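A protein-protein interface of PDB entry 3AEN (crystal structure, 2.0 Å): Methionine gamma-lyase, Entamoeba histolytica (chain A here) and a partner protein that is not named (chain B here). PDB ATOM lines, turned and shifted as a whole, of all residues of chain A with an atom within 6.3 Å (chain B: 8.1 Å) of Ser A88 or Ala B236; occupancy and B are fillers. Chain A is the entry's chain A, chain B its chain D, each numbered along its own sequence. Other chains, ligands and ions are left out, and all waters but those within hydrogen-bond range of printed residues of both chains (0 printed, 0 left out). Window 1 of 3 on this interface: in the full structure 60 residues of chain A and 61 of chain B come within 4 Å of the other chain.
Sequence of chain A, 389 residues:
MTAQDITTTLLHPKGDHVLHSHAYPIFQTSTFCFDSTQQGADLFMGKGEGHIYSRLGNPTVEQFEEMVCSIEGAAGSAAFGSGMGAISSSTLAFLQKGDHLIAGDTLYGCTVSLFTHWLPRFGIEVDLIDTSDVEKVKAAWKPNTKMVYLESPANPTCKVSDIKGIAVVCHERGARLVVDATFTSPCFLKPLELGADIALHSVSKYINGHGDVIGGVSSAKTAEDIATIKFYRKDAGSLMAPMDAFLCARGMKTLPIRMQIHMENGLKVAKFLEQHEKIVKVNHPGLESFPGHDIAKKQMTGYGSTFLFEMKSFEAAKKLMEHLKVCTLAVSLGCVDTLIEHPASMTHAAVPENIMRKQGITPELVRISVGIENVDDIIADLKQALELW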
ATOM      1  N   SER A  82     -27.530 -22.146   6.781  1.00  0.00           N
ATOM      2  CA  SER A  82     -27.963 -20.726   6.802  1.00  0.00           C
ATOM      3  C   SER A  82     -28.826 -20.492   5.547  1.00  0.00           C
ATOM      4  O   SER A  82     -28.790 -21.301   4.618  1.00  0.00           O
ATOM      5  CB  SER A  82     -26.727 -19.803   6.796  1.00  0.00           C
ATOM      6  OG  SER A  82     -25.920 -20.066   5.642  1.00  0.00           O
ATOM      7  N   GLY A  83     -29.609 -19.411   5.538  1.00  0.00           N
ATOM      8  CA  GLY A  83     -30.255 -18.908   4.342  1.00  0.00           C
ATOM      9  C   GLY A  83     -29.271 -18.754   3.198  1.00  0.00           C
ATOM     10  O   GLY A  83     -29.556 -19.181   2.076  1.00  0.00           O
ATOM     11  N   MET A  84     -28.096 -18.178   3.464  1.00  0.00           N
ATOM     12  CA  MET A  84     -27.072 -18.073   2.431  1.00  0.00           C
ATOM     13  C   MET A  84     -26.651 -19.426   1.859  1.00  0.00           C
ATOM     14  O   MET A  84     -26.344 -19.502   0.671  1.00  0.00           O
ATOM     15  CB  MET A  84     -25.844 -17.254   2.899  1.00  0.00           C
ATOM     16  CG  MET A  84     -26.111 -15.723   3.070  1.00  0.00           C
ATOM     17  SD  MET A  84     -27.230 -14.926   1.854  1.00  0.00           S
ATOM     18  CE  MET A  84     -26.338 -15.173   0.297  1.00  0.00           C
ATOM     19  N   GLY A  85     -26.601 -20.476   2.684  1.00  0.00           N
ATOM     20  CA  GLY A  85     -26.343 -21.839   2.207  1.00  0.00           C
ATOM     21  C   GLY A  85     -27.450 -22.274   1.240  1.00  0.00           C
ATOM     22  O   GLY A  85     -27.175 -22.831   0.158  1.00  0.00           O
ATOM     23  N   ALA A  86     -28.698 -22.008   1.604  1.00  0.00           N
ATOM     24  CA  ALA A  86     -29.834 -22.338   0.720  1.00  0.00           C
ATOM     25  C   ALA A  86     -29.758 -21.568  -0.623  1.00  0.00           C
ATOM     26  O   ALA A  86     -30.044 -22.134  -1.685  1.00  0.00           O
ATOM     27  CB  ALA A  86     -31.160 -22.013   1.422  1.00  0.00           C
ATOM     28  N   ILE A  87     -29.397 -20.281  -0.558  1.00  0.00           N
ATOM     29  CA  ILE A  87     -29.264 -19.442  -1.761  1.00  0.00           C
ATOM     30  C   ILE A  87     -28.128 -19.890  -2.683  1.00  0.00           C
ATOM     31  O   ILE A  87     -28.318 -20.037  -3.896  1.00  0.00           O
ATOM     32  CB  ILE A  87     -29.141 -17.948  -1.398  1.00  0.00           C
ATOM     33  CG1 ILE A  87     -30.448 -17.500  -0.759  1.00  0.00           C
ATOM     34  CG2 ILE A  87     -28.834 -17.067  -2.688  1.00  0.00           C
ATOM     35  CD1 ILE A  87     -30.380 -16.094  -0.040  1.00  0.00           C
ATOM     36  N   SER A  88     -26.946 -20.090  -2.107  1.00  0.00           N
ATOM     37  CA  SER A  88     -25.809 -20.592  -2.857  1.00  0.00           C
ATOM     38  C   SER A  88     -26.153 -21.921  -3.553  1.00  0.00           C
ATOM     39  O   SER A  88     -25.879 -22.145  -4.768  1.00  0.00           O
ATOM     40  CB  SER A  88     -24.677 -20.831  -1.866  1.00  0.00           C
ATOM     41  OG  SER A  88     -23.903 -19.674  -1.818  1.00  0.00           O
ATOM     42  N   SER A  89     -26.778 -22.802  -2.779  1.00  0.00           N
ATOM     43  CA  SER A  89     -27.068 -24.163  -3.291  1.00  0.00           C
ATOM     44  C   SER A  89     -28.233 -24.207  -4.267  1.00  0.00           C
ATOM     45  O   SER A  89     -28.374 -25.204  -4.968  1.00  0.00           O
ATOM     46  CB  SER A  89     -27.293 -25.190  -2.135  1.00  0.00           C
ATOM     47  OG  SER A  89     -26.240 -25.121  -1.150  1.00  0.00           O
ATOM     48  N   SER A  90     -29.077 -23.175  -4.305  1.00  0.00           N
ATOM     49  CA  SER A  90     -30.241 -23.148  -5.208  1.00  0.00           C
ATOM     50  C   SER A  90     -29.890 -22.429  -6.525  1.00  0.00           C
ATOM     51  O   SER A  90     -30.703 -22.403  -7.469  1.00  0.00           O
ATOM     52  CB  SER A  90     -31.467 -22.451  -4.559  1.00  0.00           C
ATOM     53  OG  SER A  90     -31.913 -23.168  -3.401  1.00  0.00           O
ATOM     54  N   THR A  91     -28.701 -21.830  -6.567  1.00  0.00           N
ATOM     55  CA  THR A  91     -28.277 -21.068  -7.728  1.00  0.00           C
ATOM     56  C   THR A  91     -27.102 -21.797  -8.365  1.00  0.00           C
ATOM     57  O   THR A  91     -27.194 -22.220  -9.518  1.00  0.00           O
ATOM     58  CB  THR A  91     -27.902 -19.574  -7.374  1.00  0.00           C
ATOM     59  OG1 THR A  91     -27.004 -19.534  -6.256  1.00  0.00           O
ATOM     60  CG2 THR A  91     -29.146 -18.761  -7.007  1.00  0.00           C
ATOM     61  N   LEU A  92     -26.021 -21.968  -7.601  1.00  0.00           N
ATOM     62  CA  LEU A  92     -24.800 -22.577  -8.111  1.00  0.00           C
ATOM     63  C   LEU A  92     -24.919 -24.099  -8.347  1.00  0.00           C
ATOM     64  O   LEU A  92     -24.080 -24.691  -9.024  1.00  0.00           O
ATOM     65  CB  LEU A  92     -23.619 -22.257  -7.180  1.00  0.00           C
ATOM     66  CG  LEU A  92     -23.135 -20.814  -7.131  1.00  0.00           C
ATOM     67  CD1 LEU A  92     -22.103 -20.578  -5.998  1.00  0.00           C
ATOM     68  CD2 LEU A  92     -22.552 -20.449  -8.465  1.00  0.00           C
ATOM     69  N   ALA A  93     -25.968 -24.724  -7.815  1.00  0.00           N
ATOM     70  CA  ALA A  93     -26.271 -26.116  -8.210  1.00  0.00           C
ATOM     71  C   ALA A  93     -26.668 -26.238  -9.684  1.00  0.00           C
ATOM     72  O   ALA A  93     -26.486 -27.297 -10.275  1.00  0.00           O
ATOM     73  CB  ALA A  93     -27.323 -26.738  -7.313  1.00  0.00           C
ATOM     74  N   LEU A 114     -23.040 -12.267  -3.069  1.00  0.00           N
ATOM     75  CA  LEU A 114     -22.885 -13.562  -3.732  1.00  0.00           C
ATOM     76  C   LEU A 114     -22.992 -13.407  -5.248  1.00  0.00           C
ATOM     77  O   LEU A 114     -22.155 -13.933  -5.983  1.00  0.00           O
ATOM     78  CB  LEU A 114     -23.921 -14.576  -3.206  1.00  0.00           C
ATOM     79  CG  LEU A 114     -24.013 -15.972  -3.881  1.00  0.00           C
ATOM     80  CD1 LEU A 114     -22.797 -16.876  -3.628  1.00  0.00           C
ATOM     81  CD2 LEU A 114     -25.291 -16.657  -3.403  1.00  0.00           C
ATOM     82  N   TRP A 118     -19.086 -13.355  -6.249  1.00  0.00           N
ATOM     83  CA  TRP A 118     -18.711 -14.743  -6.525  1.00  0.00           C
ATOM     84  C   TRP A 118     -19.188 -15.296  -7.854  1.00  0.00           C
ATOM     85  O   TRP A 118     -18.391 -15.879  -8.554  1.00  0.00           O
ATOM     86  CB  TRP A 118     -19.044 -15.676  -5.356  1.00  0.00           C
ATOM     87  CG  TRP A 118     -18.397 -15.254  -4.088  1.00  0.00           C
ATOM     88  CD1 TRP A 118     -19.000 -14.637  -3.015  1.00  0.00           C
ATOM     89  CD2 TRP A 118     -17.010 -15.396  -3.745  1.00  0.00           C
ATOM     90  NE1 TRP A 118     -18.074 -14.403  -2.029  1.00  0.00           N
ATOM     91  CE2 TRP A 118     -16.849 -14.861  -2.440  1.00  0.00           C
ATOM     92  CE3 TRP A 118     -15.888 -15.936  -4.413  1.00  0.00           C
ATOM     93  CZ2 TRP A 118     -15.610 -14.830  -1.784  1.00  0.00           C
ATOM     94  CZ3 TRP A 118     -14.641 -15.919  -3.753  1.00  0.00           C
ATOM     95  CH2 TRP A 118     -14.527 -15.374  -2.447  1.00  0.00           C
ATOM     96  N   TYR A 232     -25.404 -30.953  -4.774  1.00  0.00           N
ATOM     97  CA  TYR A 232     -24.539 -29.810  -4.494  1.00  0.00           C
ATOM     98  C   TYR A 232     -24.183 -29.685  -3.000  1.00  0.00           C
ATOM     99  O   TYR A 232     -22.991 -29.542  -2.641  1.00  0.00           O
ATOM    100  CB  TYR A 232     -25.195 -28.534  -4.986  1.00  0.00           C
ATOM    101  CG  TYR A 232     -24.347 -27.303  -4.836  1.00  0.00           C
ATOM    102  CD1 TYR A 232     -24.415 -26.523  -3.689  1.00  0.00           C
ATOM    103  CD2 TYR A 232     -23.476 -26.905  -5.869  1.00  0.00           C
ATOM    104  CE1 TYR A 232     -23.623 -25.382  -3.565  1.00  0.00           C
ATOM    105  CE2 TYR A 232     -22.714 -25.790  -5.756  1.00  0.00           C
ATOM    106  CZ  TYR A 232     -22.775 -25.028  -4.598  1.00  0.00           C
ATOM    107  OH  TYR A 232     -21.991 -23.891  -4.521  1.00  0.00           O
ATOM    108  N   SER A 238     -22.973 -27.006   3.278  1.00  0.00           N
ATOM    109  CA  SER A 238     -23.819 -26.215   4.199  1.00  0.00           C
ATOM    110  C   SER A 238     -24.938 -27.056   4.793  1.00  0.00           C
ATOM    111  O   SER A 238     -25.966 -27.276   4.161  1.00  0.00           O
ATOM    112  CB  SER A 238     -24.380 -24.937   3.575  1.00  0.00           C
ATOM    113  OG  SER A 238     -25.182 -24.241   4.547  1.00  0.00           O
ATOM    114  N   ARG B  55     -23.814 -15.777  11.673  1.00  0.00           N
ATOM    115  CA  ARG B  55     -23.124 -16.094  10.417  1.00  0.00           C
ATOM    116  C   ARG B  55     -21.805 -15.320  10.215  1.00  0.00           C
ATOM    117  O   ARG B  55     -20.835 -15.876   9.651  1.00  0.00           O
ATOM    118  CB  ARG B  55     -24.037 -15.966   9.193  1.00  0.00           C
ATOM    119  CG  ARG B  55     -23.309 -16.205   7.825  1.00  0.00           C
ATOM    120  CD  ARG B  55     -24.303 -16.547   6.678  1.00  0.00           C
ATOM    121  NE  ARG B  55     -25.446 -15.647   6.705  1.00  0.00           N
ATOM    122  CZ  ARG B  55     -25.408 -14.348   6.400  1.00  0.00           C
ATOM    123  NH1 ARG B  55     -24.276 -13.788   5.947  1.00  0.00           N
ATOM    124  NH2 ARG B  55     -26.524 -13.627   6.467  1.00  0.00           N
ATOM    125  N   PHE B  80     -16.661 -24.623   9.969  1.00  0.00           N
ATOM    126  CA  PHE B  80     -17.706 -24.830   8.999  1.00  0.00           C
ATOM    127  C   PHE B  80     -18.634 -25.931   9.431  1.00  0.00           C
ATOM    128  O   PHE B  80     -18.338 -26.662  10.369  1.00  0.00           O
ATOM    129  CB  PHE B  80     -17.093 -25.223   7.640  1.00  0.00           C
ATOM    130  CG  PHE B  80     -16.189 -24.187   7.079  1.00  0.00           C
ATOM    131  CD1 PHE B  80     -16.681 -23.232   6.200  1.00  0.00           C
ATOM    132  CD2 PHE B  80     -14.824 -24.167   7.428  1.00  0.00           C
ATOM    133  CE1 PHE B  80     -15.835 -22.269   5.659  1.00  0.00           C
ATOM    134  CE2 PHE B  80     -13.985 -23.194   6.892  1.00  0.00           C
ATOM    135  CZ  PHE B  80     -14.502 -22.226   6.022  1.00  0.00           C
ATOM    136  N   GLY B  85     -17.537 -28.296   3.541  1.00  0.00           N
ATOM    137  CA  GLY B  85     -17.632 -26.818   3.632  1.00  0.00           C
ATOM    138  C   GLY B  85     -16.267 -26.163   3.770  1.00  0.00           C
ATOM    139  O   GLY B  85     -15.993 -25.141   3.121  1.00  0.00           O
ATOM    140  N   SER B  88     -14.479 -26.762   0.154  1.00  0.00           N
ATOM    141  CA  SER B  88     -14.979 -25.907  -0.896  1.00  0.00           C
ATOM    142  C   SER B  88     -14.702 -24.409  -0.616  1.00  0.00           C
ATOM    143  O   SER B  88     -14.403 -23.654  -1.544  1.00  0.00           O
ATOM    144  CB  SER B  88     -16.436 -26.262  -1.269  1.00  0.00           C
ATOM    145  OG  SER B  88     -17.275 -26.031  -0.183  1.00  0.00           O
ATOM    146  N   SER B  89     -14.703 -24.000   0.649  1.00  0.00           N
ATOM    147  CA  SER B  89     -14.312 -22.632   1.002  1.00  0.00           C
ATOM    148  C   SER B  89     -12.813 -22.355   0.915  1.00  0.00           C
ATOM    149  O   SER B  89     -12.429 -21.193   0.790  1.00  0.00           O
ATOM    150  CB  SER B  89     -14.819 -22.243   2.401  1.00  0.00           C
ATOM    151  OG  SER B  89     -16.210 -22.527   2.518  1.00  0.00           O
ATOM    152  N   LEU B  92     -12.613 -22.608  -3.635  1.00  0.00           N
ATOM    153  CA  LEU B  92     -13.410 -21.669  -4.432  1.00  0.00           C
ATOM    154  C   LEU B  92     -13.413 -20.249  -3.900  1.00  0.00           C
ATOM    155  O   LEU B  92     -13.977 -19.355  -4.527  1.00  0.00           O
ATOM    156  CB  LEU B  92     -14.864 -22.154  -4.553  1.00  0.00           C
ATOM    157  CG  LEU B  92     -14.997 -23.460  -5.313  1.00  0.00           C
ATOM    158  CD1 LEU B  92     -16.371 -24.108  -5.076  1.00  0.00           C
ATOM    159  CD2 LEU B  92     -14.722 -23.217  -6.797  1.00  0.00           C
ATOM    160  N   PHE B 122     -17.430 -24.189 -13.207  1.00  0.00           N
ATOM    161  CA  PHE B 122     -17.111 -22.809 -12.852  1.00  0.00           C
ATOM    162  C   PHE B 122     -15.907 -22.301 -13.635  1.00  0.00           C
ATOM    163  O   PHE B 122     -15.396 -21.208 -13.356  1.00  0.00           O
ATOM    164  CB  PHE B 122     -16.874 -22.686 -11.334  1.00  0.00           C
ATOM    165  CG  PHE B 122     -18.044 -23.157 -10.494  1.00  0.00           C
ATOM    166  CD1 PHE B 122     -17.832 -23.729  -9.243  1.00  0.00           C
ATOM    167  CD2 PHE B 122     -19.349 -23.027 -10.958  1.00  0.00           C
ATOM    168  CE1 PHE B 122     -18.909 -24.178  -8.464  1.00  0.00           C
ATOM    169  CE2 PHE B 122     -20.422 -23.470 -10.199  1.00  0.00           C
ATOM    170  CZ  PHE B 122     -20.197 -24.057  -8.940  1.00  0.00           C
ATOM    171  N   ILE B 229     -11.268 -16.423   3.158  1.00  0.00           N
ATOM    172  CA  ILE B 229     -12.018 -17.626   3.483  1.00  0.00           C
ATOM    173  C   ILE B 229     -13.315 -17.303   4.246  1.00  0.00           C
ATOM    174  O   ILE B 229     -14.370 -17.849   3.932  1.00  0.00           O
ATOM    175  CB  ILE B 229     -11.155 -18.662   4.244  1.00  0.00           C
ATOM    176  CG1 ILE B 229     -10.142 -19.304   3.291  1.00  0.00           C
ATOM    177  CG2 ILE B 229     -12.004 -19.742   4.843  1.00  0.00           C
ATOM    178  CD1 ILE B 229      -8.977 -20.015   3.998  1.00  0.00           C
ATOM    179  N   LYS B 230     -13.242 -16.400   5.217  1.00  0.00           N
ATOM    180  CA  LYS B 230     -14.437 -16.043   5.989  1.00  0.00           C
ATOM    181  C   LYS B 230     -15.429 -15.199   5.180  1.00  0.00           C
ATOM    182  O   LYS B 230     -16.640 -15.240   5.420  1.00  0.00           O
ATOM    183  CB  LYS B 230     -14.039 -15.360   7.292  1.00  0.00           C
ATOM    184  CG  LYS B 230     -13.354 -16.329   8.229  1.00  0.00           C
ATOM    185  CD  LYS B 230     -13.019 -15.710   9.592  1.00  0.00           C
ATOM    186  CE  LYS B 230     -12.567 -16.828  10.574  1.00  0.00           C
ATOM    187  NZ  LYS B 230     -12.117 -16.337  11.903  1.00  0.00           N
ATOM    188  N   PHE B 231     -14.909 -14.457   4.211  1.00  0.00           N
ATOM    189  CA  PHE B 231     -15.742 -13.629   3.359  1.00  0.00           C
ATOM    190  C   PHE B 231     -16.557 -14.525   2.425  1.00  0.00           C
ATOM    191  O   PHE B 231     -17.742 -14.275   2.189  1.00  0.00           O
ATOM    192  CB  PHE B 231     -14.907 -12.614   2.560  1.00  0.00           C
ATOM    193  CG  PHE B 231     -15.745 -11.582   1.845  1.00  0.00           C
ATOM    194  CD1 PHE B 231     -16.097 -10.383   2.483  1.00  0.00           C
ATOM    195  CD2 PHE B 231     -16.188 -11.800   0.546  1.00  0.00           C
ATOM    196  CE1 PHE B 231     -16.879  -9.412   1.827  1.00  0.00           C
ATOM    197  CE2 PHE B 231     -16.966 -10.852  -0.126  1.00  0.00           C
ATOM    198  CZ  PHE B 231     -17.315  -9.652   0.518  1.00  0.00           C
ATOM    199  N   TYR B 232     -15.905 -15.569   1.907  1.00  0.00           N
ATOM    200  CA  TYR B 232     -16.585 -16.613   1.150  1.00  0.00           C
ATOM    201  C   TYR B 232     -17.616 -17.351   2.011  1.00  0.00           C
ATOM    202  O   TYR B 232     -18.733 -17.595   1.554  1.00  0.00           O
ATOM    203  CB  TYR B 232     -15.563 -17.609   0.580  1.00  0.00           C
ATOM    204  CG  TYR B 232     -16.162 -18.705  -0.257  1.00  0.00           C
ATOM    205  CD1 TYR B 232     -16.224 -18.593  -1.652  1.00  0.00           C
ATOM    206  CD2 TYR B 232     -16.660 -19.871   0.334  1.00  0.00           C
ATOM    207  CE1 TYR B 232     -16.777 -19.613  -2.435  1.00  0.00           C
ATOM    208  CE2 TYR B 232     -17.215 -20.899  -0.440  1.00  0.00           C
ATOM    209  CZ  TYR B 232     -17.266 -20.759  -1.827  1.00  0.00           C
ATOM    210  OH  TYR B 232     -17.795 -21.768  -2.609  1.00  0.00           O
ATOM    211  N   ARG B 233     -17.228 -17.717   3.243  1.00  0.00           N
ATOM    212  CA  ARG B 233     -18.124 -18.402   4.169  1.00  0.00           C
ATOM    213  C   ARG B 233     -19.398 -17.580   4.408  1.00  0.00           C
ATOM    214  O   ARG B 233     -20.524 -18.129   4.474  1.00  0.00           O
ATOM    215  CB  ARG B 233     -17.409 -18.717   5.505  1.00  0.00           C
ATOM    216  CG  ARG B 233     -18.247 -19.706   6.404  1.00  0.00           C
ATOM    217  CD  ARG B 233     -17.712 -19.890   7.812  1.00  0.00           C
ATOM    218  NE  ARG B 233     -17.487 -18.621   8.491  1.00  0.00           N
ATOM    219  CZ  ARG B 233     -16.817 -18.464   9.627  1.00  0.00           C
ATOM    220  NH1 ARG B 233     -16.686 -17.237  10.131  1.00  0.00           N
ATOM    221  NH2 ARG B 233     -16.271 -19.514  10.262  1.00  0.00           N
ATOM    222  N   LYS B 234     -19.221 -16.269   4.553  1.00  0.00           N
ATOM    223  CA  LYS B 234     -20.333 -15.346   4.768  1.00  0.00           C
ATOM    224  C   LYS B 234     -21.423 -15.520   3.687  1.00  0.00           C
ATOM    225  O   LYS B 234     -22.605 -15.386   3.981  1.00  0.00           O
ATOM    226  CB  LYS B 234     -19.816 -13.903   4.753  1.00  0.00           C
ATOM    227  CG  LYS B 234     -20.891 -12.820   4.765  1.00  0.00           C
ATOM    228  CD  LYS B 234     -20.250 -11.409   4.846  1.00  0.00           C
ATOM    229  CE  LYS B 234     -19.726 -10.906   3.486  1.00  0.00           C
ATOM    230  NZ  LYS B 234     -20.737 -10.902   2.380  1.00  0.00           N
ATOM    231  N   ASP B 235     -20.999 -15.749   2.441  1.00  0.00           N
ATOM    232  CA  ASP B 235     -21.910 -15.830   1.288  1.00  0.00           C
ATOM    233  C   ASP B 235     -22.337 -17.261   0.911  1.00  0.00           C
ATOM    234  O   ASP B 235     -23.467 -17.467   0.428  1.00  0.00           O
ATOM    235  CB  ASP B 235     -21.277 -15.138   0.061  1.00  0.00           C
ATOM    236  CG  ASP B 235     -21.142 -13.602   0.240  1.00  0.00           C
ATOM    237  OD1 ASP B 235     -20.415 -12.965  -0.569  1.00  0.00           O
ATOM    238  OD2 ASP B 235     -21.748 -13.036   1.185  1.00  0.00           O
ATOM    239  N   ALA B 236     -21.423 -18.219   1.095  1.00  0.00           N
ATOM    240  CA  ALA B 236     -21.657 -19.646   0.844  1.00  0.00           C
ATOM    241  C   ALA B 236     -22.442 -20.326   1.970  1.00  0.00           C
ATOM    242  O   ALA B 236     -23.246 -21.237   1.728  1.00  0.00           O
ATOM    243  CB  ALA B 236     -20.330 -20.385   0.606  1.00  0.00           C
ATOM    244  N   GLY B 237     -22.172 -19.934   3.206  1.00  0.00           N
ATOM    245  CA  GLY B 237     -23.064 -20.289   4.323  1.00  0.00           C
ATOM    246  C   GLY B 237     -22.937 -21.631   5.027  1.00  0.00           C
ATOM    247  O   GLY B 237     -23.917 -22.090   5.664  1.00  0.00           O
ATOM    248  N   SER B 238     -21.775 -22.273   4.906  1.00  0.00           N
ATOM    249  CA  SER B 238     -21.479 -23.490   5.677  1.00  0.00           C
ATOM    250  C   SER B 238     -20.893 -23.111   7.041  1.00  0.00           C
ATOM    251  O   SER B 238     -19.685 -22.813   7.188  1.00  0.00           O
ATOM    252  CB  SER B 238     -20.562 -24.446   4.902  1.00  0.00           C
ATOM    253  OG  SER B 238     -20.238 -25.580   5.702  1.00  0.00           O
ATOM    254  N   LEU B 239     -21.771 -23.097   8.040  1.00  0.00           N
ATOM    255  CA  LEU B 239     -21.430 -22.636   9.388  1.00  0.00           C
ATOM    256  C   LEU B 239     -21.417 -23.820  10.343  1.00  0.00           C
ATOM    257  O   LEU B 239     -22.178 -24.792  10.146  1.00  0.00           O
ATOM    258  CB  LEU B 239     -22.492 -21.626   9.885  1.00  0.00           C
ATOM    259  CG  LEU B 239     -22.832 -20.488   8.913  1.00  0.00           C
ATOM    260  CD1 LEU B 239     -23.992 -19.627   9.462  1.00  0.00           C
ATOM    261  CD2 LEU B 239     -21.576 -19.612   8.663  1.00  0.00           C
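NE1 of Trp A118 sits at hydrogen-bond distance from OD1 of Asp B235, at 3.1 Å. The side-chain hydroxyl of Ser A88 sits at hydrogen-bond distance from the backbone carbonyl oxygen of Asp B235 (3.2 Å). O of Gly B237 is in hydrogen-bond range of OG of Ser A238, 2.7 Å away. The side-chain hydroxyl (OG) of Ser A82 lies within hydrogen-bond range of the backbone carbonyl oxygen (O) of Gly B237, at 2.8 Å.
The side-chain carboxylate (OD2) of Asp B235 lies within salt-bridge range of the side-chain amino group (NZ) of Lys B234. The backbone carbonyl oxygen (O) of Met A84 sits close to the side-chain hydroxyl (OG) of Ser A88, 3.5 Å away. OG of Ser A89 lies within hydrogen-bond range of O of Gly A85 (2.8 Å). The guanidinium group (NH1) of Arg B55 is in hydrogen-bond range of the backbone carbonyl oxygen (O) of Lys B234. The backbone NH of Gly A85 is in hydrogen-bond range of the side-chain hydroxyl of Ser A82, 3.1 Å away. O of Ser A88 is in hydrogen-bond range of OG1 of Thr A91 (3.2 Å).
Ser A82 touches Leu B239. CG of Met A84 touches CZ of Arg B55, 3.7 Å away. O of Asp B235 touches CB of Met A84, at 3.4 Å. Ala B236 touches Met A84. Ala B236 touches Gly A85. Gly A85 touches Gly B237 (N to CA, 3.9 Å). Ala B236 touches Ser A88. O of Leu B92 touches CZ3 of Trp A118 (3.6 Å). CZ2 of Trp A118 touches CA of Tyr B232 (3.6 Å). Ser A238 touches Ser B238.
Of the printed residues of chain B, Leu A114 touches Asp B235 (3.7 Å). Of the printed residues of chain A, Lys B234 touches Met A84. Ile B229 touches none of the printed residues of chain A. The nearest residue of chain B that does not touch Ser A88 is Gly B237 (5.3 Å). The nearest residue of chain A that does not touch Ala B236 is Ser A238 (4.3 Å).
Of the 16 printed residues of chain A, 8 touch a printed residue of chain B. Among the printed residues, no Asp or Glu carboxylate lies within 4 Å of a Lys or Arg side-chain nitrogen of the other chain.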
